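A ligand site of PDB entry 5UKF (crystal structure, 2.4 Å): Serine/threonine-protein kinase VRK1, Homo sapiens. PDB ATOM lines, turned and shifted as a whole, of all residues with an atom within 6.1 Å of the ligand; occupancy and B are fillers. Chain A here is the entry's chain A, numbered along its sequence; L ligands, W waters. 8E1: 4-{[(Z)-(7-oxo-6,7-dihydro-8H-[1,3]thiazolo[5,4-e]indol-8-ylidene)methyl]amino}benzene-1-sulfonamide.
OD1 of Asp 136 sits at hydrogen-bond distance from N of Lys 139 (2.9 Å). The backbone carbonyl oxygen (O) of Phe 47 lies within hydrogen-bond range of the side-chain amino group (NZ) of Lys 70, at 3.5 Å. The backbone carbonyl oxygen (O) of Val 68 sits at hydrogen-bond distance from the backbone NH (N) of Met 130, at 2.9 Å. The backbone carbonyl oxygen (O) of Ile 50 lies within hydrogen-bond range of the backbone NH (N) of Ile 42, at 2.9 Å.
Merely in contact with the ligand: Phe 47 (3.5 Å), Ile 50 (3.9 Å), Val 68 (3.5 Å), Met 130 (3.8 Å), Arg 132 (3.8 Å), Gly 134 (3.2 Å), Ser 135 (3.6 Å), Lys 139 (3.3 Å), Leu 183 (3.7 Å) and Val 195 (3.9 Å). Hydrophobic or aromatic side chains within 4 Å of the ligand: Phe 47, Ile 50, Val 68, Met 130, Phe 133, Leu 183 and Val 195. 13 residues have an atom within 4 Å of the ligand: Phe 47, Ile 50, Val 68, Met 130, Asp 131, Arg 132, Phe 133, Gly 134, Ser 135, Asp 136, Lys 139, Leu 183 and Val 195. Along chain A the residues within 4 Å of the ligand span positions 47 to 195. The nearest printed residue that does not touch the ligand is Asp 196 (4.2 Å).
Water W1 lies within hydrogen-bond range of a nitrogen (N1) of the ligand (2.5 Å), the side-chain hydroxyl of Tyr 86 (2.5 Å), the backbone NH of Asp 196 (2.9 Å) and the side-chain carboxylate of Glu 82 (3.0 Å).
An oxygen (O) of the ligand lies within hydrogen-bond range of the backbone NH (N) of Phe 133, 2.9 Å away. O of Asp 131 lies within hydrogen-bond range of N2 of the ligand (3.0 Å). OD1 of Asp 136 is in hydrogen-bond range of N3 of the ligand, at 3.1 Å.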
ATOM      1  N   ILE A  42      10.892  -6.743  13.391  1.00  0.00           N
ATOM      2  CA  ILE A  42      12.260  -6.336  13.059  1.00  0.00           C
ATOM      3  C   ILE A  42      12.564  -6.886  11.680  1.00  0.00           C
ATOM      4  O   ILE A  42      12.685  -8.095  11.504  1.00  0.00           O
ATOM      5  CB  ILE A  42      13.296  -6.795  14.125  1.00  0.00           C
ATOM      6  N   GLY A  43      12.596  -5.982  10.708  1.00  0.00           N
ATOM      7  CA  GLY A  43      12.872  -6.294   9.308  1.00  0.00           C
ATOM      8  C   GLY A  43      11.918  -7.281   8.658  1.00  0.00           C
ATOM      9  O   GLY A  43      10.795  -7.484   9.149  1.00  0.00           O
ATOM     10  N   GLY A  45      13.674 -10.199   6.966  1.00  0.00           N
ATOM     11  CA  GLY A  45      14.687 -11.212   6.655  1.00  0.00           C
ATOM     12  C   GLY A  45      14.191 -12.635   6.846  1.00  0.00           C
ATOM     13  O   GLY A  45      13.247 -12.883   7.598  1.00  0.00           O
ATOM     14  N   PHE A  47      14.671 -15.087   8.610  1.00  0.00           N
ATOM     15  CA  PHE A  47      14.983 -15.620   9.919  1.00  0.00           C
ATOM     16  C   PHE A  47      13.722 -15.999  10.674  1.00  0.00           C
ATOM     17  O   PHE A  47      13.784 -16.447  11.818  1.00  0.00           O
ATOM     18  CB  PHE A  47      15.702 -14.541  10.714  1.00  0.00           C
ATOM     19  CG  PHE A  47      17.174 -14.490  10.468  1.00  0.00           C
ATOM     20  CD1 PHE A  47      17.961 -15.617  10.585  1.00  0.00           C
ATOM     21  CD2 PHE A  47      17.799 -13.278  10.198  1.00  0.00           C
ATOM     22  CE1 PHE A  47      19.324 -15.555  10.392  1.00  0.00           C
ATOM     23  CE2 PHE A  47      19.162 -13.217  10.006  1.00  0.00           C
ATOM     24  CZ  PHE A  47      19.929 -14.350  10.108  1.00  0.00           C
ATOM     25  N   ILE A  50      10.089 -12.263  13.807  1.00  0.00           N
ATOM     26  CA  ILE A  50      10.804 -11.583  14.902  1.00  0.00           C
ATOM     27  C   ILE A  50      10.237 -10.169  15.162  1.00  0.00           C
ATOM     28  O   ILE A  50      10.121  -9.370  14.235  1.00  0.00           O
ATOM     29  CB  ILE A  50      12.355 -11.582  14.674  1.00  0.00           C
ATOM     30  CG1 ILE A  50      12.907 -13.019  14.493  1.00  0.00           C
ATOM     31  CG2 ILE A  50      13.075 -10.872  15.826  1.00  0.00           C
ATOM     32  CD1 ILE A  50      14.282 -13.102  13.885  1.00  0.00           C
ATOM     33  N   VAL A  68      14.235  -9.165  21.679  1.00  0.00           N
ATOM     34  CA  VAL A  68      13.419  -9.561  20.573  1.00  0.00           C
ATOM     35  C   VAL A  68      12.661 -10.813  20.951  1.00  0.00           C
ATOM     36  O   VAL A  68      13.076 -11.589  21.786  1.00  0.00           O
ATOM     37  CB  VAL A  68      14.230  -9.894  19.300  1.00  0.00           C
ATOM     38  CG1 VAL A  68      14.836  -8.651  18.686  1.00  0.00           C
ATOM     39  CG2 VAL A  68      15.265 -10.964  19.574  1.00  0.00           C
ATOM     40  N   LYS A  70      11.134 -14.083  19.088  1.00  0.00           N
ATOM     41  CA  LYS A  70      11.155 -14.923  17.894  1.00  0.00           C
ATOM     42  C   LYS A  70      10.022 -15.901  18.094  1.00  0.00           C
ATOM     43  O   LYS A  70       9.938 -16.548  19.122  1.00  0.00           O
ATOM     44  CB  LYS A  70      12.481 -15.664  17.798  1.00  0.00           C
ATOM     45  CG  LYS A  70      12.712 -16.357  16.474  1.00  0.00           C
ATOM     46  CD  LYS A  70      14.171 -16.731  16.303  1.00  0.00           C
ATOM     47  CE  LYS A  70      14.388 -17.598  15.081  1.00  0.00           C
ATOM     48  NZ  LYS A  70      13.158 -18.316  14.668  1.00  0.00           N
ATOM     49  N   GLU A  82      16.566 -25.116  17.974  1.00  0.00           N
ATOM     50  CA  GLU A  82      17.183 -23.851  18.313  1.00  0.00           C
ATOM     51  C   GLU A  82      16.922 -23.494  19.764  1.00  0.00           C
ATOM     52  O   GLU A  82      17.791 -22.989  20.448  1.00  0.00           O
ATOM     53  CB  GLU A  82      16.663 -22.757  17.388  1.00  0.00           C
ATOM     54  CG  GLU A  82      17.337 -21.409  17.546  1.00  0.00           C
ATOM     55  CD  GLU A  82      17.135 -20.522  16.352  1.00  0.00           C
ATOM     56  OE1 GLU A  82      15.981 -20.281  15.972  1.00  0.00           O
ATOM     57  OE2 GLU A  82      18.128 -20.073  15.766  1.00  0.00           O
ATOM     58  N   TYR A  86      19.628 -23.056  23.022  1.00  0.00           N
ATOM     59  CA  TYR A  86      19.637 -21.840  23.830  1.00  0.00           C
ATOM     60  C   TYR A  86      19.424 -22.130  25.307  1.00  0.00           C
ATOM     61  O   TYR A  86      20.063 -21.532  26.150  1.00  0.00           O
ATOM     62  CB  TYR A  86      18.612 -20.837  23.287  1.00  0.00           C
ATOM     63  CG  TYR A  86      19.133 -20.017  22.130  1.00  0.00           C
ATOM     64  CD1 TYR A  86      20.299 -19.298  22.237  1.00  0.00           C
ATOM     65  CD2 TYR A  86      18.460 -19.985  20.930  1.00  0.00           C
ATOM     66  CE1 TYR A  86      20.782 -18.567  21.175  1.00  0.00           C
ATOM     67  CE2 TYR A  86      18.929 -19.259  19.867  1.00  0.00           C
ATOM     68  CZ  TYR A  86      20.094 -18.543  19.999  1.00  0.00           C
ATOM     69  OH  TYR A  86      20.566 -17.811  18.957  1.00  0.00           O
ATOM     70  N   PRO A 110      24.268 -15.398  21.469  1.00  0.00           N
ATOM     71  CA  PRO A 110      23.157 -14.569  21.920  1.00  0.00           C
ATOM     72  C   PRO A 110      22.571 -15.099  23.206  1.00  0.00           C
ATOM     73  O   PRO A 110      22.427 -16.295  23.352  1.00  0.00           O
ATOM     74  CB  PRO A 110      22.136 -14.684  20.794  1.00  0.00           C
ATOM     75  CG  PRO A 110      22.898 -15.204  19.632  1.00  0.00           C
ATOM     76  CD  PRO A 110      23.941 -16.091  20.224  1.00  0.00           C
ATOM     77  N   MET A 130      15.122 -13.145  23.109  1.00  0.00           N
ATOM     78  CA  MET A 130      16.555 -13.094  22.934  1.00  0.00           C
ATOM     79  C   MET A 130      17.139 -11.696  22.916  1.00  0.00           C
ATOM     80  O   MET A 130      16.422 -10.718  22.833  1.00  0.00           O
ATOM     81  CB  MET A 130      16.934 -13.754  21.605  1.00  0.00           C
ATOM     82  CG  MET A 130      16.267 -15.087  21.333  1.00  0.00           C
ATOM     83  SD  MET A 130      17.194 -16.432  22.079  1.00  0.00           S
ATOM     84  CE  MET A 130      18.862 -15.877  21.764  1.00  0.00           C
ATOM     85  N   ASP A 131      18.465 -11.654  22.913  1.00  0.00           N
ATOM     86  CA  ASP A 131      19.249 -10.442  22.837  1.00  0.00           C
ATOM     87  C   ASP A 131      18.993  -9.839  21.473  1.00  0.00           C
ATOM     88  O   ASP A 131      18.923 -10.548  20.497  1.00  0.00           O
ATOM     89  CB  ASP A 131      20.724 -10.804  22.891  1.00  0.00           C
ATOM     90  CG  ASP A 131      21.328 -10.650  24.262  1.00  0.00           C
ATOM     91  OD1 ASP A 131      20.648 -10.126  25.164  1.00  0.00           O
ATOM     92  OD2 ASP A 131      22.485 -11.058  24.450  1.00  0.00           O
ATOM     93  N   ARG A 132      18.885  -8.530  21.408  1.00  0.00           N
ATOM     94  CA  ARG A 132      18.647  -7.827  20.149  1.00  0.00           C
ATOM     95  C   ARG A 132      19.955  -7.398  19.476  1.00  0.00           C
ATOM     96  O   ARG A 132      20.896  -6.976  20.146  1.00  0.00           O
ATOM     97  CB  ARG A 132      17.778  -6.600  20.413  1.00  0.00           C
ATOM     98  CG  ARG A 132      17.379  -5.844  19.179  1.00  0.00           C
ATOM     99  CD  ARG A 132      17.629  -4.406  19.409  1.00  0.00           C
ATOM    100  NE  ARG A 132      16.821  -3.582  18.515  1.00  0.00           N
ATOM    101  CZ  ARG A 132      16.551  -2.309  18.725  1.00  0.00           C
ATOM    102  NH1 ARG A 132      16.984  -1.708  19.819  1.00  0.00           N
ATOM    103  NH2 ARG A 132      15.819  -1.631  17.851  1.00  0.00           N
ATOM    104  N   PHE A 133      19.980  -7.477  18.151  1.00  0.00           N
ATOM    105  CA  PHE A 133      21.154  -7.088  17.385  1.00  0.00           C
ATOM    106  C   PHE A 133      20.789  -6.122  16.284  1.00  0.00           C
ATOM    107  O   PHE A 133      19.633  -5.965  15.937  1.00  0.00           O
ATOM    108  CB  PHE A 133      21.815  -8.320  16.770  1.00  0.00           C
ATOM    109  CG  PHE A 133      22.110  -9.389  17.774  1.00  0.00           C
ATOM    110  CD1 PHE A 133      23.062  -9.185  18.734  1.00  0.00           C
ATOM    111  CD2 PHE A 133      21.410 -10.576  17.756  1.00  0.00           C
ATOM    112  CE1 PHE A 133      23.325 -10.150  19.670  1.00  0.00           C
ATOM    113  CE2 PHE A 133      21.667 -11.542  18.679  1.00  0.00           C
ATOM    114  CZ  PHE A 133      22.633 -11.333  19.641  1.00  0.00           C
ATOM    115  N   GLY A 134      21.802  -5.463  15.744  1.00  0.00           N
ATOM    116  CA  GLY A 134      21.613  -4.529  14.671  1.00  0.00           C
ATOM    117  C   GLY A 134      21.866  -5.200  13.343  1.00  0.00           C
ATOM    118  O   GLY A 134      21.370  -6.287  13.087  1.00  0.00           O
ATOM    119  N   SER A 135      22.671  -4.562  12.508  1.00  0.00           N
ATOM    120  CA  SER A 135      22.975  -5.090  11.189  1.00  0.00           C
ATOM    121  C   SER A 135      23.806  -6.364  11.139  1.00  0.00           C
ATOM    122  O   SER A 135      24.627  -6.622  12.013  1.00  0.00           O
ATOM    123  CB  SER A 135      23.672  -4.015  10.353  1.00  0.00           C
ATOM    124  OG  SER A 135      23.546  -4.280   8.973  1.00  0.00           O
ATOM    125  N   ASP A 136      23.575  -7.149  10.094  1.00  0.00           N
ATOM    126  CA  ASP A 136      24.353  -8.353   9.883  1.00  0.00           C
ATOM    127  C   ASP A 136      25.659  -7.985   9.171  1.00  0.00           C
ATOM    128  O   ASP A 136      25.794  -6.916   8.593  1.00  0.00           O
ATOM    129  CB  ASP A 136      23.561  -9.380   9.082  1.00  0.00           C
ATOM    130  CG  ASP A 136      23.345  -8.974   7.638  1.00  0.00           C
ATOM    131  OD1 ASP A 136      23.746  -7.863   7.266  1.00  0.00           O
ATOM    132  OD2 ASP A 136      22.754  -9.763   6.880  1.00  0.00           O
ATOM    133  N   LEU A 137      26.604  -8.890   9.218  1.00  0.00           N
ATOM    134  CA  LEU A 137      27.893  -8.657   8.575  1.00  0.00           C
ATOM    135  C   LEU A 137      27.790  -8.526   7.057  1.00  0.00           C
ATOM    136  O   LEU A 137      28.525  -7.761   6.463  1.00  0.00           O
ATOM    137  CB  LEU A 137      28.896  -9.733   8.949  1.00  0.00           C
ATOM    138  CG  LEU A 137      29.870  -9.331  10.056  1.00  0.00           C
ATOM    139  CD1 LEU A 137      31.182 -10.054   9.886  1.00  0.00           C
ATOM    140  CD2 LEU A 137      30.073  -7.834  10.037  1.00  0.00           C
ATOM    141  N   LYS A 139      25.562  -7.121   5.117  1.00  0.00           N
ATOM    142  CA  LYS A 139      25.205  -5.792   4.638  1.00  0.00           C
ATOM    143  C   LYS A 139      26.397  -4.861   4.673  1.00  0.00           C
ATOM    144  O   LYS A 139      26.612  -4.076   3.767  1.00  0.00           O
ATOM    145  CB  LYS A 139      24.073  -5.206   5.489  1.00  0.00           C
ATOM    146  CG  LYS A 139      22.763  -5.086   4.756  1.00  0.00           C
ATOM    147  CD  LYS A 139      21.736  -6.049   5.304  1.00  0.00           C
ATOM    148  CE  LYS A 139      21.324  -7.080   4.262  1.00  0.00           C
ATOM    149  NZ  LYS A 139      19.895  -6.935   3.880  1.00  0.00           N
ATOM    150  N   LEU A 183      25.784 -11.196  13.407  1.00  0.00           N
ATOM    151  CA  LEU A 183      25.074  -9.977  13.704  1.00  0.00           C
ATOM    152  C   LEU A 183      25.884  -9.138  14.648  1.00  0.00           C
ATOM    153  O   LEU A 183      26.653  -9.636  15.447  1.00  0.00           O
ATOM    154  CB  LEU A 183      23.707 -10.295  14.320  1.00  0.00           C
ATOM    155  CG  LEU A 183      22.532 -10.456  13.359  1.00  0.00           C
ATOM    156  CD1 LEU A 183      22.963 -11.149  12.088  1.00  0.00           C
ATOM    157  CD2 LEU A 183      21.394 -11.221  14.010  1.00  0.00           C
ATOM    158  N   VAL A 195      24.513 -16.324  15.103  1.00  0.00           N
ATOM    159  CA  VAL A 195      23.077 -16.653  15.240  1.00  0.00           C
ATOM    160  C   VAL A 195      22.694 -17.843  14.343  1.00  0.00           C
ATOM    161  O   VAL A 195      23.493 -18.300  13.515  1.00  0.00           O
ATOM    162  CB  VAL A 195      22.154 -15.410  14.991  1.00  0.00           C
ATOM    163  CG1 VAL A 195      22.443 -14.281  15.974  1.00  0.00           C
ATOM    164  CG2 VAL A 195      22.234 -14.901  13.539  1.00  0.00           C
ATOM    165  N   ASP A 196      21.456 -18.294  14.493  1.00  0.00           N
ATOM    166  CA  ASP A 196      20.888 -19.395  13.713  1.00  0.00           C
ATOM    167  C   ASP A 196      21.379 -20.775  14.132  1.00  0.00           C
ATOM    168  O   ASP A 196      22.352 -21.299  13.599  1.00  0.00           O
ATOM    169  CB  ASP A 196      21.084 -19.173  12.219  1.00  0.00           C
ATOM    170  CG  ASP A 196      20.040 -19.893  11.393  1.00  0.00           C
ATOM    171  OD1 ASP A 196      19.488 -20.902  11.873  1.00  0.00           O
ATOM    172  OD2 ASP A 196      19.770 -19.466  10.263  1.00  0.00           O
HETATM  173  C1  8E1 L   1      18.650  -6.362  11.358  1.00  0.00           C
HETATM  174  N1  8E1 L   1      18.327 -15.694  15.613  1.00  0.00           N
HETATM  175  O1  8E1 L   1      18.660  -6.763   7.760  1.00  0.00           O
HETATM  176  S1  8E1 L   1      19.565  -6.314   8.784  1.00  0.00           S
HETATM  177  C2  8E1 L   1      19.075  -7.117  10.275  1.00  0.00           C
HETATM  178  O2  8E1 L   1      19.668  -4.923   9.052  1.00  0.00           O
HETATM  179  C3  8E1 L   1      19.132  -8.498  10.362  1.00  0.00           C
HETATM  180  C4  8E1 L   1      18.742  -9.125  11.528  1.00  0.00           C
HETATM  181  C5  8E1 L   1      18.312  -8.377  12.614  1.00  0.00           C
HETATM  182  C6  8E1 L   1      17.824 -10.341  14.007  1.00  0.00           C
HETATM  183  C7  8E1 L   1      17.955 -10.759  15.312  1.00  0.00           C
HETATM  184  C8  8E1 L   1      18.087 -12.080  15.925  1.00  0.00           C
HETATM  185  C9  8E1 L   1      18.172 -11.887  17.307  1.00  0.00           C
HETATM  186  C10 8E1 L   1      18.311 -12.965  18.169  1.00  0.00           C
HETATM  187  C11 8E1 L   1      18.369 -14.284  17.654  1.00  0.00           C
HETATM  188  C12 8E1 L   1      18.286 -14.464  16.278  1.00  0.00           C
HETATM  189  C13 8E1 L   1      18.146 -13.369  15.429  1.00  0.00           C
HETATM  190  C14 8E1 L   1      18.200 -15.512  14.332  1.00  0.00           C
HETATM  191  C15 8E1 L   1      17.994  -9.792  16.419  1.00  0.00           C
HETATM  192  N3  8E1 L   1      21.022  -6.831   8.382  1.00  0.00           N
HETATM  193  C   8E1 L   1      18.260  -6.988  12.524  1.00  0.00           C
HETATM  194  N   8E1 L   1      17.915  -9.014  13.807  1.00  0.00           N
HETATM  195  O   8E1 L   1      17.956  -8.567  16.364  1.00  0.00           O
HETATM  196  N2  8E1 L   1      18.094 -10.517  17.562  1.00  0.00           N
HETATM  197  S   8E1 L   1      18.075 -13.894  13.783  1.00  0.00           S
HETATM  198  O   HOH W   1      19.578 -17.550  16.638  1.00  0.00           O
